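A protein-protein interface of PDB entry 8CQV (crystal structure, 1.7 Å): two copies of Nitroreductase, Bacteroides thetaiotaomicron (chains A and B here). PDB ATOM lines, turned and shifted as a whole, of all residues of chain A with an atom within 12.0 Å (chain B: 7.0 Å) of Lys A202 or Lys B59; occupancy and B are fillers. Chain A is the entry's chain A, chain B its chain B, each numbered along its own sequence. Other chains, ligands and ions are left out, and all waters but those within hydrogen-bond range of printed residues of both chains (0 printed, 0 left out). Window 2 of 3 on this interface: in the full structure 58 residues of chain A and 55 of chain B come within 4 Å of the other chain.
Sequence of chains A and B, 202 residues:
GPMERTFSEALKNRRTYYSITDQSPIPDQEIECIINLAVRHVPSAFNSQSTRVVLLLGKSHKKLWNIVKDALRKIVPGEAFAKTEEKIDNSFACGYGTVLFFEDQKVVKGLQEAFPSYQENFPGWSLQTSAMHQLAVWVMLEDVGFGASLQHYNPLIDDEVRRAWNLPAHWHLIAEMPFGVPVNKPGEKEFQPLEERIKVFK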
ATOM      1  N   ILE A 198      -1.031 -20.572  13.341  1.00  0.00           N
ATOM      2  CA  ILE A 198      -1.835 -21.786  13.298  1.00  0.00           C
ATOM      3  C   ILE A 198      -2.089 -22.187  14.735  1.00  0.00           C
ATOM      4  O   ILE A 198      -1.134 -22.220  15.537  1.00  0.00           O
ATOM      5  CB  ILE A 198      -1.135 -22.905  12.522  1.00  0.00           C
ATOM      6  CG1 ILE A 198      -0.827 -22.487  11.079  1.00  0.00           C
ATOM      7  CG2 ILE A 198      -1.940 -24.183  12.584  1.00  0.00           C
ATOM      8  CD1 ILE A 198       0.222 -23.336  10.383  1.00  0.00           C
ATOM      9  N   LYS A 199      -3.365 -22.455  15.076  1.00  0.00           N
ATOM     10  CA  LYS A 199      -3.731 -23.033  16.375  1.00  0.00           C
ATOM     11  C   LYS A 199      -4.521 -24.306  16.121  1.00  0.00           C
ATOM     12  O   LYS A 199      -5.299 -24.389  15.156  1.00  0.00           O
ATOM     13  CB  LYS A 199      -4.583 -22.060  17.183  1.00  0.00           C
ATOM     14  CG  LYS A 199      -3.907 -20.730  17.455  1.00  0.00           C
ATOM     15  CD  LYS A 199      -2.699 -20.851  18.340  1.00  0.00           C
ATOM     16  CE  LYS A 199      -1.749 -19.706  18.102  1.00  0.00           C
ATOM     17  NZ  LYS A 199      -0.699 -19.705  19.139  1.00  0.00           N
ATOM     18  N   VAL A 200      -4.303 -25.303  16.974  1.00  0.00           N
ATOM     19  CA  VAL A 200      -5.021 -26.577  16.877  1.00  0.00           C
ATOM     20  C   VAL A 200      -5.637 -26.835  18.241  1.00  0.00           C
ATOM     21  O   VAL A 200      -4.942 -26.731  19.241  1.00  0.00           O
ATOM     22  CB  VAL A 200      -4.147 -27.758  16.419  1.00  0.00           C
ATOM     23  CG1 VAL A 200      -4.986 -29.036  16.237  1.00  0.00           C
ATOM     24  CG2 VAL A 200      -3.396 -27.440  15.162  1.00  0.00           C
ATOM     25  N   PHE A 201      -6.958 -27.077  18.285  1.00  0.00           N
ATOM     26  CA  PHE A 201      -7.685 -27.349  19.523  1.00  0.00           C
ATOM     27  C   PHE A 201      -8.470 -28.626  19.326  1.00  0.00           C
ATOM     28  O   PHE A 201      -9.085 -28.770  18.298  1.00  0.00           O
ATOM     29  CB  PHE A 201      -8.672 -26.213  19.781  1.00  0.00           C
ATOM     30  CG  PHE A 201      -7.985 -24.890  20.026  1.00  0.00           C
ATOM     31  CD1 PHE A 201      -7.373 -24.646  21.248  1.00  0.00           C
ATOM     32  CD2 PHE A 201      -7.966 -23.907  19.066  1.00  0.00           C
ATOM     33  CE1 PHE A 201      -6.722 -23.442  21.456  1.00  0.00           C
ATOM     34  CE2 PHE A 201      -7.352 -22.689  19.307  1.00  0.00           C
ATOM     35  CZ  PHE A 201      -6.739 -22.462  20.509  1.00  0.00           C
ATOM     36  N   LYS A 202      -8.532 -29.525  20.332  1.00  0.00           N
ATOM     37  CA  LYS A 202      -9.315 -30.739  20.187  1.00  0.00           C
ATOM     38  C   LYS A 202     -10.304 -30.856  21.358  1.00  0.00           C
ATOM     39  O   LYS A 202     -10.791 -29.799  21.817  1.00  0.00           O
ATOM     40  CB  LYS A 202      -8.377 -31.931  19.999  1.00  0.00           C
ATOM     41  CG  LYS A 202      -9.073 -33.236  19.608  1.00  0.00           C
ATOM     42  CD  LYS A 202      -8.192 -34.181  18.812  1.00  0.00           C
ATOM     43  CE  LYS A 202      -8.872 -35.506  18.513  1.00  0.00           C
ATOM     44  NZ  LYS A 202      -7.887 -36.577  18.226  1.00  0.00           N
ATOM     45  OXT LYS A 202     -10.590 -32.001  21.764  1.00  0.00           O
ATOM     46  N   ASP B  28      -3.869 -37.059  13.269  1.00  0.00           N
ATOM     47  CA  ASP B  28      -4.109 -35.627  13.453  1.00  0.00           C
ATOM     48  C   ASP B  28      -2.908 -34.753  13.096  1.00  0.00           C
ATOM     49  O   ASP B  28      -3.121 -33.650  12.578  1.00  0.00           O
ATOM     50  CB  ASP B  28      -4.472 -35.291  14.886  1.00  0.00           C
ATOM     51  CG  ASP B  28      -5.789 -35.876  15.337  1.00  0.00           C
ATOM     52  OD1 ASP B  28      -6.598 -36.277  14.441  1.00  0.00           O
ATOM     53  OD2 ASP B  28      -5.935 -36.005  16.591  1.00  0.00           O
ATOM     54  N   LEU B  55      -7.454 -25.059  13.438  1.00  0.00           N
ATOM     55  CA  LEU B  55      -7.978 -26.393  13.202  1.00  0.00           C
ATOM     56  C   LEU B  55      -8.683 -26.874  14.475  1.00  0.00           C
ATOM     57  O   LEU B  55      -8.059 -26.901  15.536  1.00  0.00           O
ATOM     58  CB  LEU B  55      -6.803 -27.315  12.867  1.00  0.00           C
ATOM     59  CG  LEU B  55      -7.163 -28.777  12.683  1.00  0.00           C
ATOM     60  CD1 LEU B  55      -8.151 -28.967  11.580  1.00  0.00           C
ATOM     61  CD2 LEU B  55      -5.925 -29.635  12.418  1.00  0.00           C
ATOM     62  N   LEU B  56      -9.977 -27.230  14.343  1.00  0.00           N
ATOM     63  CA  LEU B  56     -10.789 -27.716  15.442  1.00  0.00           C
ATOM     64  C   LEU B  56     -11.084 -29.173  15.174  1.00  0.00           C
ATOM     65  O   LEU B  56     -11.685 -29.535  14.159  1.00  0.00           O
ATOM     66  CB  LEU B  56     -12.109 -26.946  15.564  1.00  0.00           C
ATOM     67  CG  LEU B  56     -11.965 -25.447  15.741  1.00  0.00           C
ATOM     68  CD1 LEU B  56     -13.345 -24.765  15.892  1.00  0.00           C
ATOM     69  CD2 LEU B  56     -11.073 -25.113  16.911  1.00  0.00           C
ATOM     70  N   LEU B  57     -10.759 -30.011  16.168  1.00  0.00           N
ATOM     71  CA  LEU B  57     -10.998 -31.444  16.056  1.00  0.00           C
ATOM     72  C   LEU B  57     -11.792 -31.877  17.276  1.00  0.00           C
ATOM     73  O   LEU B  57     -11.903 -31.115  18.250  1.00  0.00           O
ATOM     74  CB  LEU B  57      -9.628 -32.141  16.115  1.00  0.00           C
ATOM     75  CG  LEU B  57      -8.676 -31.824  14.987  1.00  0.00           C
ATOM     76  CD1 LEU B  57      -7.325 -32.457  15.236  1.00  0.00           C
ATOM     77  CD2 LEU B  57      -9.275 -32.306  13.690  1.00  0.00           C
ATOM     78  N   GLY B  58     -12.405 -33.047  17.172  1.00  0.00           N
ATOM     79  CA  GLY B  58     -13.008 -33.701  18.319  1.00  0.00           C
ATOM     80  C   GLY B  58     -14.086 -32.840  18.959  1.00  0.00           C
ATOM     81  O   GLY B  58     -14.925 -32.261  18.246  1.00  0.00           O
ATOM     82  N   LYS B  59     -14.028 -32.646  20.275  1.00  0.00           N
ATOM     83  CA  LYS B  59     -15.054 -31.835  20.937  1.00  0.00           C
ATOM     84  C   LYS B  59     -15.036 -30.351  20.522  1.00  0.00           C
ATOM     85  O   LYS B  59     -16.083 -29.725  20.571  1.00  0.00           O
ATOM     86  CB  LYS B  59     -15.065 -31.969  22.465  1.00  0.00           C
ATOM     87  CG  LYS B  59     -14.051 -31.153  23.237  1.00  0.00           C
ATOM     88  CD  LYS B  59     -13.959 -31.625  24.718  1.00  0.00           C
ATOM     89  CE  LYS B  59     -12.976 -30.804  25.516  1.00  0.00           C
ATOM     90  NZ  LYS B  59     -11.599 -31.010  25.009  1.00  0.00           N
ATOM     91  N   SER B  60     -13.888 -29.771  20.133  1.00  0.00           N
ATOM     92  CA  SER B  60     -13.844 -28.401  19.635  1.00  0.00           C
ATOM     93  C   SER B  60     -14.622 -28.274  18.305  1.00  0.00           C
ATOM     94  O   SER B  60     -15.329 -27.313  18.123  1.00  0.00           O
ATOM     95  CB  SER B  60     -12.457 -27.914  19.474  1.00  0.00           C
ATOM     96  OG  SER B  60     -11.877 -27.655  20.746  1.00  0.00           O
ATOM     97  N   HIS B  61     -14.542 -29.271  17.432  1.00  0.00           N
ATOM     98  CA  HIS B  61     -15.331 -29.307  16.226  1.00  0.00           C
ATOM     99  C   HIS B  61     -16.810 -29.324  16.556  1.00  0.00           C
ATOM    100  O   HIS B  61     -17.619 -28.587  15.966  1.00  0.00           O
ATOM    101  CB  HIS B  61     -14.902 -30.503  15.386  1.00  0.00           C
ATOM    102  CG  HIS B  61     -15.897 -30.884  14.368  1.00  0.00           C
ATOM    103  ND1 HIS B  61     -16.042 -30.241  13.156  1.00  0.00           N
ATOM    104  CD2 HIS B  61     -16.785 -31.911  14.388  1.00  0.00           C
ATOM    105  CE1 HIS B  61     -17.024 -30.857  12.504  1.00  0.00           C
ATOM    106  NE2 HIS B  61     -17.494 -31.879  13.253  1.00  0.00           N
ATOM    107  N   LYS B  62     -17.199 -30.188  17.523  1.00  0.00           N
ATOM    108  CA  LYS B  62     -18.599 -30.222  17.929  1.00  0.00           C
ATOM    109  C   LYS B  62     -19.055 -28.892  18.520  1.00  0.00           C
ATOM    110  O   LYS B  62     -20.128 -28.387  18.161  1.00  0.00           O
ATOM    111  CB  LYS B  62     -18.863 -31.382  18.877  1.00  0.00           C
ATOM    112  CG  LYS B  62     -18.612 -32.756  18.272  1.00  0.00           C
ATOM    113  CD  LYS B  62     -19.630 -33.160  17.214  1.00  0.00           C
ATOM    114  CE  LYS B  62     -19.972 -34.647  17.197  1.00  0.00           C
ATOM    115  NZ  LYS B  62     -21.176 -34.968  18.014  1.00  0.00           N
ATOM    116  N   LYS B  63     -18.230 -28.279  19.351  1.00  0.00           N
ATOM    117  CA  LYS B  63     -18.544 -26.977  19.906  1.00  0.00           C
ATOM    118  C   LYS B  63     -18.754 -25.918  18.823  1.00  0.00           C
ATOM    119  O   LYS B  63     -19.673 -25.152  18.946  1.00  0.00           O
ATOM    120  CB  LYS B  63     -17.439 -26.531  20.853  1.00  0.00           C
ATOM    121  CG  LYS B  63     -17.626 -25.167  21.509  1.00  0.00           C
ATOM    122  CD  LYS B  63     -18.860 -25.065  22.406  1.00  0.00           C
ATOM    123  CE  LYS B  63     -18.832 -23.881  23.354  1.00  0.00           C
ATOM    124  NZ  LYS B  63     -20.214 -23.537  23.696  1.00  0.00           N
ATOM    125  N   LEU B  64     -17.932 -25.909  17.768  1.00  0.00           N
ATOM    126  CA  LEU B  64     -18.104 -24.891  16.726  1.00  0.00           C
ATOM    127  C   LEU B  64     -19.527 -24.981  16.147  1.00  0.00           C
ATOM    128  O   LEU B  64     -20.178 -23.947  15.985  1.00  0.00           O
ATOM    129  CB  LEU B  64     -16.997 -25.124  15.675  1.00  0.00           C
ATOM    130  CG  LEU B  64     -16.864 -24.155  14.478  1.00  0.00           C
ATOM    131  CD1 LEU B  64     -17.922 -24.351  13.445  1.00  0.00           C
ATOM    132  CD2 LEU B  64     -16.819 -22.703  15.003  1.00  0.00           C
ATOM    133  N   ASN B  66     -22.209 -26.343  17.467  1.00  0.00           N
ATOM    134  CA  ASN B  66     -23.121 -25.899  18.537  1.00  0.00           C
ATOM    135  C   ASN B  66     -23.227 -24.373  18.593  1.00  0.00           C
ATOM    136  O   ASN B  66     -24.339 -23.866  18.776  1.00  0.00           O
ATOM    137  CB  ASN B  66     -22.726 -26.499  19.900  1.00  0.00           C
ATOM    138  CG  ASN B  66     -22.999 -27.980  19.949  1.00  0.00           C
ATOM    139  OD1 ASN B  66     -23.812 -28.464  19.156  1.00  0.00           O
ATOM    140  ND2 ASN B  66     -22.480 -28.653  20.971  1.00  0.00           N
ATOM    141  N   TYR B  96     -15.160 -34.916  11.159  1.00  0.00           N
ATOM    142  CA  TYR B  96     -14.006 -35.151  11.997  1.00  0.00           C
ATOM    143  C   TYR B  96     -13.495 -33.830  12.573  1.00  0.00           C
ATOM    144  O   TYR B  96     -12.981 -33.777  13.697  1.00  0.00           O
ATOM    145  CB  TYR B  96     -12.924 -35.898  11.218  1.00  0.00           C
ATOM    146  CG  TYR B  96     -11.775 -36.368  12.069  1.00  0.00           C
ATOM    147  CD1 TYR B  96     -11.885 -37.513  12.855  1.00  0.00           C
ATOM    148  CD2 TYR B  96     -10.599 -35.638  12.165  1.00  0.00           C
ATOM    149  CE1 TYR B  96     -10.852 -37.919  13.706  1.00  0.00           C
ATOM    150  CE2 TYR B  96      -9.557 -36.045  12.990  1.00  0.00           C
ATOM    151  CZ  TYR B  96      -9.703 -37.177  13.802  1.00  0.00           C
ATOM    152  OH  TYR B  96      -8.686 -37.655  14.582  1.00  0.00           O
ATOM    153  N   TRP B 165     -12.243 -19.914  21.935  1.00  0.00           N
ATOM    154  CA  TRP B 165     -10.885 -20.413  21.808  1.00  0.00           C
ATOM    155  C   TRP B 165      -9.861 -19.341  22.182  1.00  0.00           C
ATOM    156  O   TRP B 165      -8.692 -19.538  21.869  1.00  0.00           O
ATOM    157  CB  TRP B 165     -10.689 -21.002  20.410  1.00  0.00           C
ATOM    158  CG  TRP B 165     -11.364 -22.337  20.308  1.00  0.00           C
ATOM    159  CD1 TRP B 165     -10.938 -23.527  20.793  1.00  0.00           C
ATOM    160  CD2 TRP B 165     -12.681 -22.582  19.793  1.00  0.00           C
ATOM    161  NE1 TRP B 165     -11.893 -24.489  20.634  1.00  0.00           N
ATOM    162  CE2 TRP B 165     -12.946 -23.967  19.938  1.00  0.00           C
ATOM    163  CE3 TRP B 165     -13.599 -21.780  19.113  1.00  0.00           C
ATOM    164  CZ2 TRP B 165     -14.167 -24.552  19.514  1.00  0.00           C
ATOM    165  CZ3 TRP B 165     -14.793 -22.347  18.700  1.00  0.00           C
ATOM    166  CH2 TRP B 165     -15.082 -23.704  18.936  1.00  0.00           C
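N of Leu B57 is in hydrogen-bond range of O of Phe A201, 3.0 Å away.
The chain-end carboxylate (O) of Lys A202 is in salt-bridge range of the side-chain amino group (NZ) of Lys B59, 3.5 Å away.
The backbone carbonyl oxygen of Leu B55 is in hydrogen-bond range of the backbone NH of Phe A201, 3.0 Å away.
O of Lys A202 lies within hydrogen-bond range of OG of Ser B60.
OD2 of Asp B28 is in salt-bridge range of NZ of Lys A202.
The backbone carbonyl oxygen of Lys A199 is in hydrogen-bond range of the backbone NH of Leu B55.
The side-chain hydroxyl of Ser B60 lies within hydrogen-bond range of the indole nitrogen of Trp B165 (3.2 Å).
The side-chain carboxylate (OD1) of Asp B28 lies within hydrogen-bond range of the side-chain hydroxyl (OH) of Tyr B96 (2.5 Å).
Val A200 touches Leu B55.
Leu B56 touches Phe A201 (CA to O, 3.5 Å).
CB of Phe A201 touches OG of Ser B60, 3.6 Å away.
CD1 of Trp B165 touches CG of Phe A201 (3.3 Å).
CA of Lys A202 touches O of Leu B57, 3.3 Å away.
NZ of Lys A202 touches OH of Tyr B96 (3.9 Å).
Ile A198 touches none of the printed residues of chain B.
Printed residues of chain B within 4 Å of Lys A199: Leu B55 (2.8 Å).
Of the printed residues of chain B, Val A200 touches Leu B55.
Of the printed residues of chain B, Phe A201 touches Leu B55 (3.0 Å), Leu B56 (3.5 Å), Leu B57 (3.0 Å), Ser B60 (3.6 Å) and Trp B165 (3.3 Å).
Printed residues of chain A within 4 Å of Leu B55: Lys A199, Val A200 and Phe A201.
Of chain A, only Phe A201 (3.5 Å) comes within 4 Å of Leu B56.
Of chain A, only Phe A201 and Lys A202 come within 4 Å of Leu B57.
No residue of chain A comes within 4 Å of Gly B58.
Of the printed residues of chain A, Lys B59 touches Lys A202 (3.5 Å).
Ser B60 touches just these residues of chain A: Phe A201 and Lys A202.
His B61 touches none of the printed residues of chain A.
Lys B62 touches none of the printed residues of chain A.
Of the printed residues of chain A, Tyr B96 touches Lys A202 (3.9 Å).
The nearest printed residue of chain B that does not touch Lys A199 is Leu B56 (5.5 Å).
Hydrophobic or aromatic side chains of chain A that line the printed part of chain B: Val A200 and Phe A201.
Along chain A the printed residues that touch a printed residue of chain B span positions 199 to 202.
Among the printed residues, 12 pairs touch across the chains.
No position is printed for both chains.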
